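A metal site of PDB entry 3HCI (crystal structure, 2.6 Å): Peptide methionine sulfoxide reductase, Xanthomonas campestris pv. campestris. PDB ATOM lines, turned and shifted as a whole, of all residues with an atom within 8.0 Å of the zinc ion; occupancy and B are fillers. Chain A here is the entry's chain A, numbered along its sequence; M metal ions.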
ATOM      1  N   PRO A   9       0.148  34.436   3.537  1.00  0.00           N
ATOM      2  CA  PRO A   9      -0.378  34.303   4.898  1.00  0.00           C
ATOM      3  C   PRO A   9       0.755  34.262   5.930  1.00  0.00           C
ATOM      4  O   PRO A   9       1.834  33.734   5.639  1.00  0.00           O
ATOM      5  CB  PRO A   9      -1.132  32.971   4.855  1.00  0.00           C
ATOM      6  CG  PRO A   9      -0.536  32.215   3.734  1.00  0.00           C
ATOM      7  CD  PRO A   9      -0.158  33.255   2.708  1.00  0.00           C
ATOM      8  N   ARG A  14      -1.132  30.385   8.012  1.00  0.00           N
ATOM      9  CA  ARG A  14      -0.557  29.257   7.318  1.00  0.00           C
ATOM     10  C   ARG A  14      -0.863  27.944   8.051  1.00  0.00           C
ATOM     11  O   ARG A  14      -1.442  27.031   7.462  1.00  0.00           O
ATOM     12  CB  ARG A  14       0.959  29.455   7.160  1.00  0.00           C
ATOM     13  CG  ARG A  14       1.593  28.489   6.202  1.00  0.00           C
ATOM     14  CD  ARG A  14       3.104  28.643   6.082  1.00  0.00           C
ATOM     15  NE  ARG A  14       3.621  27.570   5.235  1.00  0.00           N
ATOM     16  CZ  ARG A  14       3.494  27.527   3.908  1.00  0.00           C
ATOM     17  NH1 ARG A  14       2.874  28.516   3.263  1.00  0.00           N
ATOM     18  NH2 ARG A  14       3.986  26.503   3.223  1.00  0.00           N
ATOM     19  N   LEU A  17      -4.525  26.828   8.127  1.00  0.00           N
ATOM     20  CA  LEU A  17      -4.972  26.197   6.887  1.00  0.00           C
ATOM     21  C   LEU A  17      -4.342  24.820   6.678  1.00  0.00           C
ATOM     22  O   LEU A  17      -5.029  23.895   6.253  1.00  0.00           O
ATOM     23  CB  LEU A  17      -4.670  27.103   5.691  1.00  0.00           C
ATOM     24  CG  LEU A  17      -5.332  28.482   5.715  1.00  0.00           C
ATOM     25  CD1 LEU A  17      -4.772  29.348   4.623  1.00  0.00           C
ATOM     26  CD2 LEU A  17      -6.854  28.400   5.627  1.00  0.00           C
ATOM     27  N   LEU A  29       1.502  19.128  -1.390  1.00  0.00           N
ATOM     28  CA  LEU A  29       1.556  20.593  -1.270  1.00  0.00           C
ATOM     29  C   LEU A  29       2.781  21.095  -0.513  1.00  0.00           C
ATOM     30  O   LEU A  29       3.415  22.056  -0.940  1.00  0.00           O
ATOM     31  CB  LEU A  29       0.263  21.157  -0.653  1.00  0.00           C
ATOM     32  CG  LEU A  29      -0.993  21.235  -1.520  1.00  0.00           C
ATOM     33  CD1 LEU A  29      -2.248  21.180  -0.673  1.00  0.00           C
ATOM     34  CD2 LEU A  29      -1.002  22.483  -2.388  1.00  0.00           C
ATOM     35  N   THR A  52      -8.595  26.525  -7.927  1.00  0.00           N
ATOM     36  CA  THR A  52      -7.976  27.307  -6.865  1.00  0.00           C
ATOM     37  C   THR A  52      -6.896  26.513  -6.139  1.00  0.00           C
ATOM     38  O   THR A  52      -6.896  25.278  -6.159  1.00  0.00           O
ATOM     39  CB  THR A  52      -9.031  27.765  -5.827  1.00  0.00           C
ATOM     40  OG1 THR A  52      -9.753  26.619  -5.345  1.00  0.00           O
ATOM     41  CG2 THR A  52     -10.004  28.757  -6.446  1.00  0.00           C
ATOM     42  N   CYS A  53      -5.981  27.229  -5.508  1.00  0.00           N
ATOM     43  CA  CYS A  53      -4.993  26.624  -4.646  1.00  0.00           C
ATOM     44  C   CYS A  53      -5.680  25.902  -3.471  1.00  0.00           C
ATOM     45  O   CYS A  53      -6.502  26.497  -2.781  1.00  0.00           O
ATOM     46  CB  CYS A  53      -4.043  27.711  -4.136  1.00  0.00           C
ATOM     47  SG  CYS A  53      -2.865  27.147  -2.912  1.00  0.00           S
ATOM     48  N   ARG A  54      -5.361  24.625  -3.275  1.00  0.00           N
ATOM     49  CA  ARG A  54      -6.000  23.824  -2.226  1.00  0.00           C
ATOM     50  C   ARG A  54      -5.702  24.374  -0.830  1.00  0.00           C
ATOM     51  O   ARG A  54      -6.512  24.223   0.083  1.00  0.00           O
ATOM     52  CB  ARG A  54      -5.627  22.326  -2.365  1.00  0.00           C
ATOM     53  CG  ARG A  54      -6.051  21.342  -1.227  1.00  0.00           C
ATOM     54  CD  ARG A  54      -7.567  21.237  -0.955  1.00  0.00           C
ATOM     55  NE  ARG A  54      -7.914  21.934   0.282  1.00  0.00           N
ATOM     56  CZ  ARG A  54      -8.145  21.352   1.468  1.00  0.00           C
ATOM     57  NH1 ARG A  54      -8.103  20.030   1.607  1.00  0.00           N
ATOM     58  NH2 ARG A  54      -8.428  22.094   2.525  1.00  0.00           N
ATOM     59  N   LEU A  55      -4.565  25.057  -0.678  1.00  0.00           N
ATOM     60  CA  LEU A  55      -4.202  25.637   0.622  1.00  0.00           C
ATOM     61  C   LEU A  55      -4.860  27.003   0.893  1.00  0.00           C
ATOM     62  O   LEU A  55      -5.633  27.130   1.845  1.00  0.00           O
ATOM     63  CB  LEU A  55      -2.668  25.708   0.804  1.00  0.00           C
ATOM     64  CG  LEU A  55      -2.190  25.942   2.252  1.00  0.00           C
ATOM     65  CD1 LEU A  55      -2.761  24.907   3.214  1.00  0.00           C
ATOM     66  CD2 LEU A  55      -0.678  25.944   2.355  1.00  0.00           C
ATOM     67  N   CYS A  56      -4.585  27.991   0.038  1.00  0.00           N
ATOM     68  CA  CYS A  56      -5.003  29.368   0.320  1.00  0.00           C
ATOM     69  C   CYS A  56      -6.145  29.911  -0.552  1.00  0.00           C
ATOM     70  O   CYS A  56      -6.565  31.057  -0.399  1.00  0.00           O
ATOM     71  CB  CYS A  56      -3.797  30.292   0.244  1.00  0.00           C
ATOM     72  SG  CYS A  56      -3.439  30.797  -1.424  1.00  0.00           S
ATOM     73  N   GLY A  57      -6.635  29.081  -1.461  1.00  0.00           N
ATOM     74  CA  GLY A  57      -7.825  29.442  -2.239  1.00  0.00           C
ATOM     75  C   GLY A  57      -7.582  30.342  -3.424  1.00  0.00           C
ATOM     76  O   GLY A  57      -8.520  30.627  -4.173  1.00  0.00           O
ATOM     77  N   LEU A  58      -6.339  30.789  -3.612  1.00  0.00           N
ATOM     78  CA  LEU A  58      -5.990  31.654  -4.728  1.00  0.00           C
ATOM     79  C   LEU A  58      -6.325  31.000  -6.055  1.00  0.00           C
ATOM     80  O   LEU A  58      -5.906  29.864  -6.312  1.00  0.00           O
ATOM     81  CB  LEU A  58      -4.506  32.038  -4.698  1.00  0.00           C
ATOM     82  CG  LEU A  58      -4.055  33.058  -5.770  1.00  0.00           C
ATOM     83  CD1 LEU A  58      -4.596  34.452  -5.482  1.00  0.00           C
ATOM     84  CD2 LEU A  58      -2.551  33.109  -5.890  1.00  0.00           C
ATOM     85  N   PRO A  59      -7.112  31.693  -6.910  1.00  0.00           N
ATOM     86  CA  PRO A  59      -7.377  31.207  -8.257  1.00  0.00           C
ATOM     87  C   PRO A  59      -6.068  30.995  -9.032  1.00  0.00           C
ATOM     88  O   PRO A  59      -5.243  31.909  -9.132  1.00  0.00           O
ATOM     89  CB  PRO A  59      -8.204  32.331  -8.869  1.00  0.00           C
ATOM     90  CG  PRO A  59      -8.893  32.939  -7.711  1.00  0.00           C
ATOM     91  CD  PRO A  59      -7.838  32.953  -6.660  1.00  0.00           C
ATOM     92  N   LEU A  60      -5.896  29.797  -9.566  1.00  0.00           N
ATOM     93  CA  LEU A  60      -4.659  29.440 -10.244  1.00  0.00           C
ATOM     94  C   LEU A  60      -4.863  29.191 -11.737  1.00  0.00           C
ATOM     95  O   LEU A  60      -4.072  29.667 -12.548  1.00  0.00           O
ATOM     96  CB  LEU A  60      -4.021  28.221  -9.576  1.00  0.00           C
ATOM     97  CG  LEU A  60      -3.524  28.375  -8.132  1.00  0.00           C
ATOM     98  CD1 LEU A  60      -3.103  27.030  -7.607  1.00  0.00           C
ATOM     99  CD2 LEU A  60      -2.386  29.376  -8.031  1.00  0.00           C
ATOM    100  N   HIS A  84      -0.055  34.865 -10.442  1.00  0.00           N
ATOM    101  CA  HIS A  84      -0.625  33.912  -9.476  1.00  0.00           C
ATOM    102  C   HIS A  84       0.158  32.623  -9.322  1.00  0.00           C
ATOM    103  O   HIS A  84       0.068  31.946  -8.299  1.00  0.00           O
ATOM    104  CB  HIS A  84      -2.081  33.604  -9.825  1.00  0.00           C
ATOM    105  CG  HIS A  84      -3.023  34.735  -9.575  1.00  0.00           C
ATOM    106  ND1 HIS A  84      -4.380  34.556  -9.418  1.00  0.00           N
ATOM    107  CD2 HIS A  84      -2.813  36.075  -9.459  1.00  0.00           C
ATOM    108  CE1 HIS A  84      -4.954  35.723  -9.220  1.00  0.00           C
ATOM    109  NE2 HIS A  84      -4.032  36.664  -9.242  1.00  0.00           N
ATOM    110  N   VAL A 101       4.757  26.971  -8.173  1.00  0.00           N
ATOM    111  CA  VAL A 101       4.169  27.102  -6.843  1.00  0.00           C
ATOM    112  C   VAL A 101       3.080  28.180  -6.829  1.00  0.00           C
ATOM    113  O   VAL A 101       3.056  29.057  -7.698  1.00  0.00           O
ATOM    114  CB  VAL A 101       5.237  27.421  -5.758  1.00  0.00           C
ATOM    115  CG1 VAL A 101       6.289  26.322  -5.697  1.00  0.00           C
ATOM    116  CG2 VAL A 101       5.883  28.798  -5.999  1.00  0.00           C
ATOM    117  N   CYS A 102       2.171  28.099  -5.860  1.00  0.00           N
ATOM    118  CA  CYS A 102       1.206  29.171  -5.639  1.00  0.00           C
ATOM    119  C   CYS A 102       1.947  30.402  -5.149  1.00  0.00           C
ATOM    120  O   CYS A 102       2.636  30.354  -4.132  1.00  0.00           O
ATOM    121  CB  CYS A 102       0.161  28.723  -4.623  1.00  0.00           C
ATOM    122  SG  CYS A 102      -0.843  30.068  -3.966  1.00  0.00           S
ATOM    123  N   ALA A 103       1.804  31.516  -5.882  1.00  0.00           N
ATOM    124  CA  ALA A 103       2.542  32.751  -5.586  1.00  0.00           C
ATOM    125  C   ALA A 103       2.241  33.337  -4.205  1.00  0.00           C
ATOM    126  O   ALA A 103       3.041  34.085  -3.653  1.00  0.00           O
ATOM    127  CB  ALA A 103       2.316  33.789  -6.661  1.00  0.00           C
ATOM    128  N   ARG A 104       1.077  33.010  -3.661  1.00  0.00           N
ATOM    129  CA  ARG A 104       0.660  33.543  -2.374  1.00  0.00           C
ATOM    130  C   ARG A 104       1.224  32.716  -1.221  1.00  0.00           C
ATOM    131  O   ARG A 104       1.933  33.242  -0.374  1.00  0.00           O
ATOM    132  CB  ARG A 104      -0.861  33.627  -2.289  1.00  0.00           C
ATOM    133  CG  ARG A 104      -1.365  34.298  -1.029  1.00  0.00           C
ATOM    134  CD  ARG A 104      -2.665  35.023  -1.277  1.00  0.00           C
ATOM    135  NE  ARG A 104      -3.816  34.131  -1.339  1.00  0.00           N
ATOM    136  CZ  ARG A 104      -5.054  34.516  -1.633  1.00  0.00           C
ATOM    137  NH1 ARG A 104      -5.312  35.783  -1.918  1.00  0.00           N
ATOM    138  NH2 ARG A 104      -6.043  33.623  -1.641  1.00  0.00           N
ATOM    139  N   CYS A 105       0.919  31.421  -1.194  1.00  0.00           N
ATOM    140  CA  CYS A 105       1.243  30.582  -0.053  1.00  0.00           C
ATOM    141  C   CYS A 105       2.458  29.697  -0.265  1.00  0.00           C
ATOM    142  O   CYS A 105       2.891  29.016   0.665  1.00  0.00           O
ATOM    143  CB  CYS A 105       0.053  29.714   0.308  1.00  0.00           C
ATOM    144  SG  CYS A 105      -0.174  28.432  -0.888  1.00  0.00           S
ATOM    145  N   ASP A 106       2.974  29.670  -1.494  1.00  0.00           N
ATOM    146  CA  ASP A 106       4.235  28.981  -1.783  1.00  0.00           C
ATOM    147  C   ASP A 106       4.099  27.443  -1.849  1.00  0.00           C
ATOM    148  O   ASP A 106       5.112  26.740  -1.895  1.00  0.00           O
ATOM    149  CB  ASP A 106       5.300  29.401  -0.758  1.00  0.00           C
ATOM    150  CG  ASP A 106       6.708  29.306  -1.309  1.00  0.00           C
ATOM    151  OD1 ASP A 106       7.514  28.517  -0.751  1.00  0.00           O
ATOM    152  OD2 ASP A 106       7.003  30.037  -2.289  1.00  0.00           O
ATOM    153  N   SER A 107       2.860  26.945  -1.885  1.00  0.00           N
ATOM    154  CA  SER A 107       2.572  25.506  -1.983  1.00  0.00           C
ATOM    155  C   SER A 107       2.999  24.883  -3.314  1.00  0.00           C
ATOM    156  O   SER A 107       2.959  25.553  -4.348  1.00  0.00           O
ATOM    157  CB  SER A 107       1.083  25.251  -1.814  1.00  0.00           C
ATOM    158  OG  SER A 107       0.672  25.494  -0.492  1.00  0.00           O
ATOM    159  N   HIS A 108       3.377  23.604  -3.280  1.00  0.00           N
ATOM    160  CA  HIS A 108       3.747  22.884  -4.492  1.00  0.00           C
ATOM    161  C   HIS A 108       2.530  22.560  -5.344  1.00  0.00           C
ATOM    162  O   HIS A 108       1.503  22.092  -4.822  1.00  0.00           O
ATOM    163  CB  HIS A 108       4.510  21.605  -4.167  1.00  0.00           C
ATOM    164  CG  HIS A 108       4.814  20.766  -5.368  1.00  0.00           C
ATOM    165  ND1 HIS A 108       5.804  21.096  -6.271  1.00  0.00           N
ATOM    166  CD2 HIS A 108       4.254  19.626  -5.822  1.00  0.00           C
ATOM    167  CE1 HIS A 108       5.846  20.189  -7.229  1.00  0.00           C
ATOM    168  NE2 HIS A 108       4.911  19.281  -6.978  1.00  0.00           N
ATOM    169  N   LEU A 109       2.631  22.795  -6.649  1.00  0.00           N
ATOM    170  CA  LEU A 109       1.536  22.540  -7.594  1.00  0.00           C
ATOM    171  C   LEU A 109       1.894  21.507  -8.666  1.00  0.00           C
ATOM    172  O   LEU A 109       1.065  20.687  -9.041  1.00  0.00           O
ATOM    173  CB  LEU A 109       1.089  23.841  -8.275  1.00  0.00           C
ATOM    174  CG  LEU A 109       0.739  25.037  -7.377  1.00  0.00           C
ATOM    175  CD1 LEU A 109       0.431  26.260  -8.234  1.00  0.00           C
ATOM    176  CD2 LEU A 109      -0.423  24.716  -6.427  1.00  0.00           C
ATOM    177  N   SER A 130      -3.406  19.183  -5.483  1.00  0.00           N
ATOM    178  CA  SER A 130      -2.976  20.553  -5.196  1.00  0.00           C
ATOM    179  C   SER A 130      -4.082  21.586  -5.459  1.00  0.00           C
ATOM    180  O   SER A 130      -3.903  22.775  -5.204  1.00  0.00           O
ATOM    181  CB  SER A 130      -1.738  20.918  -6.021  1.00  0.00           C
ATOM    182  OG  SER A 130      -0.582  20.313  -5.482  1.00  0.00           O
ATOM    183  N   LEU A 144      -8.828  32.947   3.546  1.00  0.00           N
ATOM    184  CA  LEU A 144      -8.121  34.053   4.202  1.00  0.00           C
ATOM    185  C   LEU A 144      -8.979  35.314   4.327  1.00  0.00           C
ATOM    186  O   LEU A 144      -8.516  36.346   4.810  1.00  0.00           O
ATOM    187  CB  LEU A 144      -6.807  34.384   3.476  1.00  0.00           C
ATOM    188  CG  LEU A 144      -5.700  33.316   3.450  1.00  0.00           C
ATOM    189  CD1 LEU A 144      -4.618  33.713   2.465  1.00  0.00           C
ATOM    190  CD2 LEU A 144      -5.098  33.102   4.833  1.00  0.00           C
HETATM  191 ZN    ZN M   1      -1.896  29.157  -2.200  1.00  0.00          ZN
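Four residues have an atom within 4 Å of the zinc ion: Cys 53, Cys 56, Cys 102 and Cys 105. The nearest printed residue that does not touch the zinc ion is Arg 104 (4.6 Å).
SG of Cys 102 lies close to N of Arg 104, at 3.5 Å. The side-chain sulfur of Cys 56 sits close to the backbone NH of Leu 58 (3.6 Å). The backbone carbonyl oxygen (O) of Cys 105 lies within hydrogen-bond range of the guanidinium group (NH1) of Arg 14, at 2.6 Å. The guanidinium group (NH2) of Arg 104 lies within hydrogen-bond range of the backbone carbonyl oxygen (O) of Cys 56 (2.9 Å). N of Cys 53 is in hydrogen-bond range of O of Leu 58. N of Cys 102 is in hydrogen-bond range of O of Ser 107 (3.1 Å). The side-chain hydroxyl (OG) of Ser 107 sits close to the side-chain sulfur (SG) of Cys 105 (3.1 Å). N of Leu 55 lies close to SG of Cys 53, 3.5 Å away.
The zinc ion is bound by the side-chain sulfur (SG) of Cys 102 (2.2 Å), the side-chain sulfur (SG) of Cys 105 (2.3 Å), the side-chain sulfur (SG) of Cys 53 (2.3 Å) and the side-chain sulfur (SG) of Cys 56 (2.4 Å). The zinc ion has four donor atoms within binding distance.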
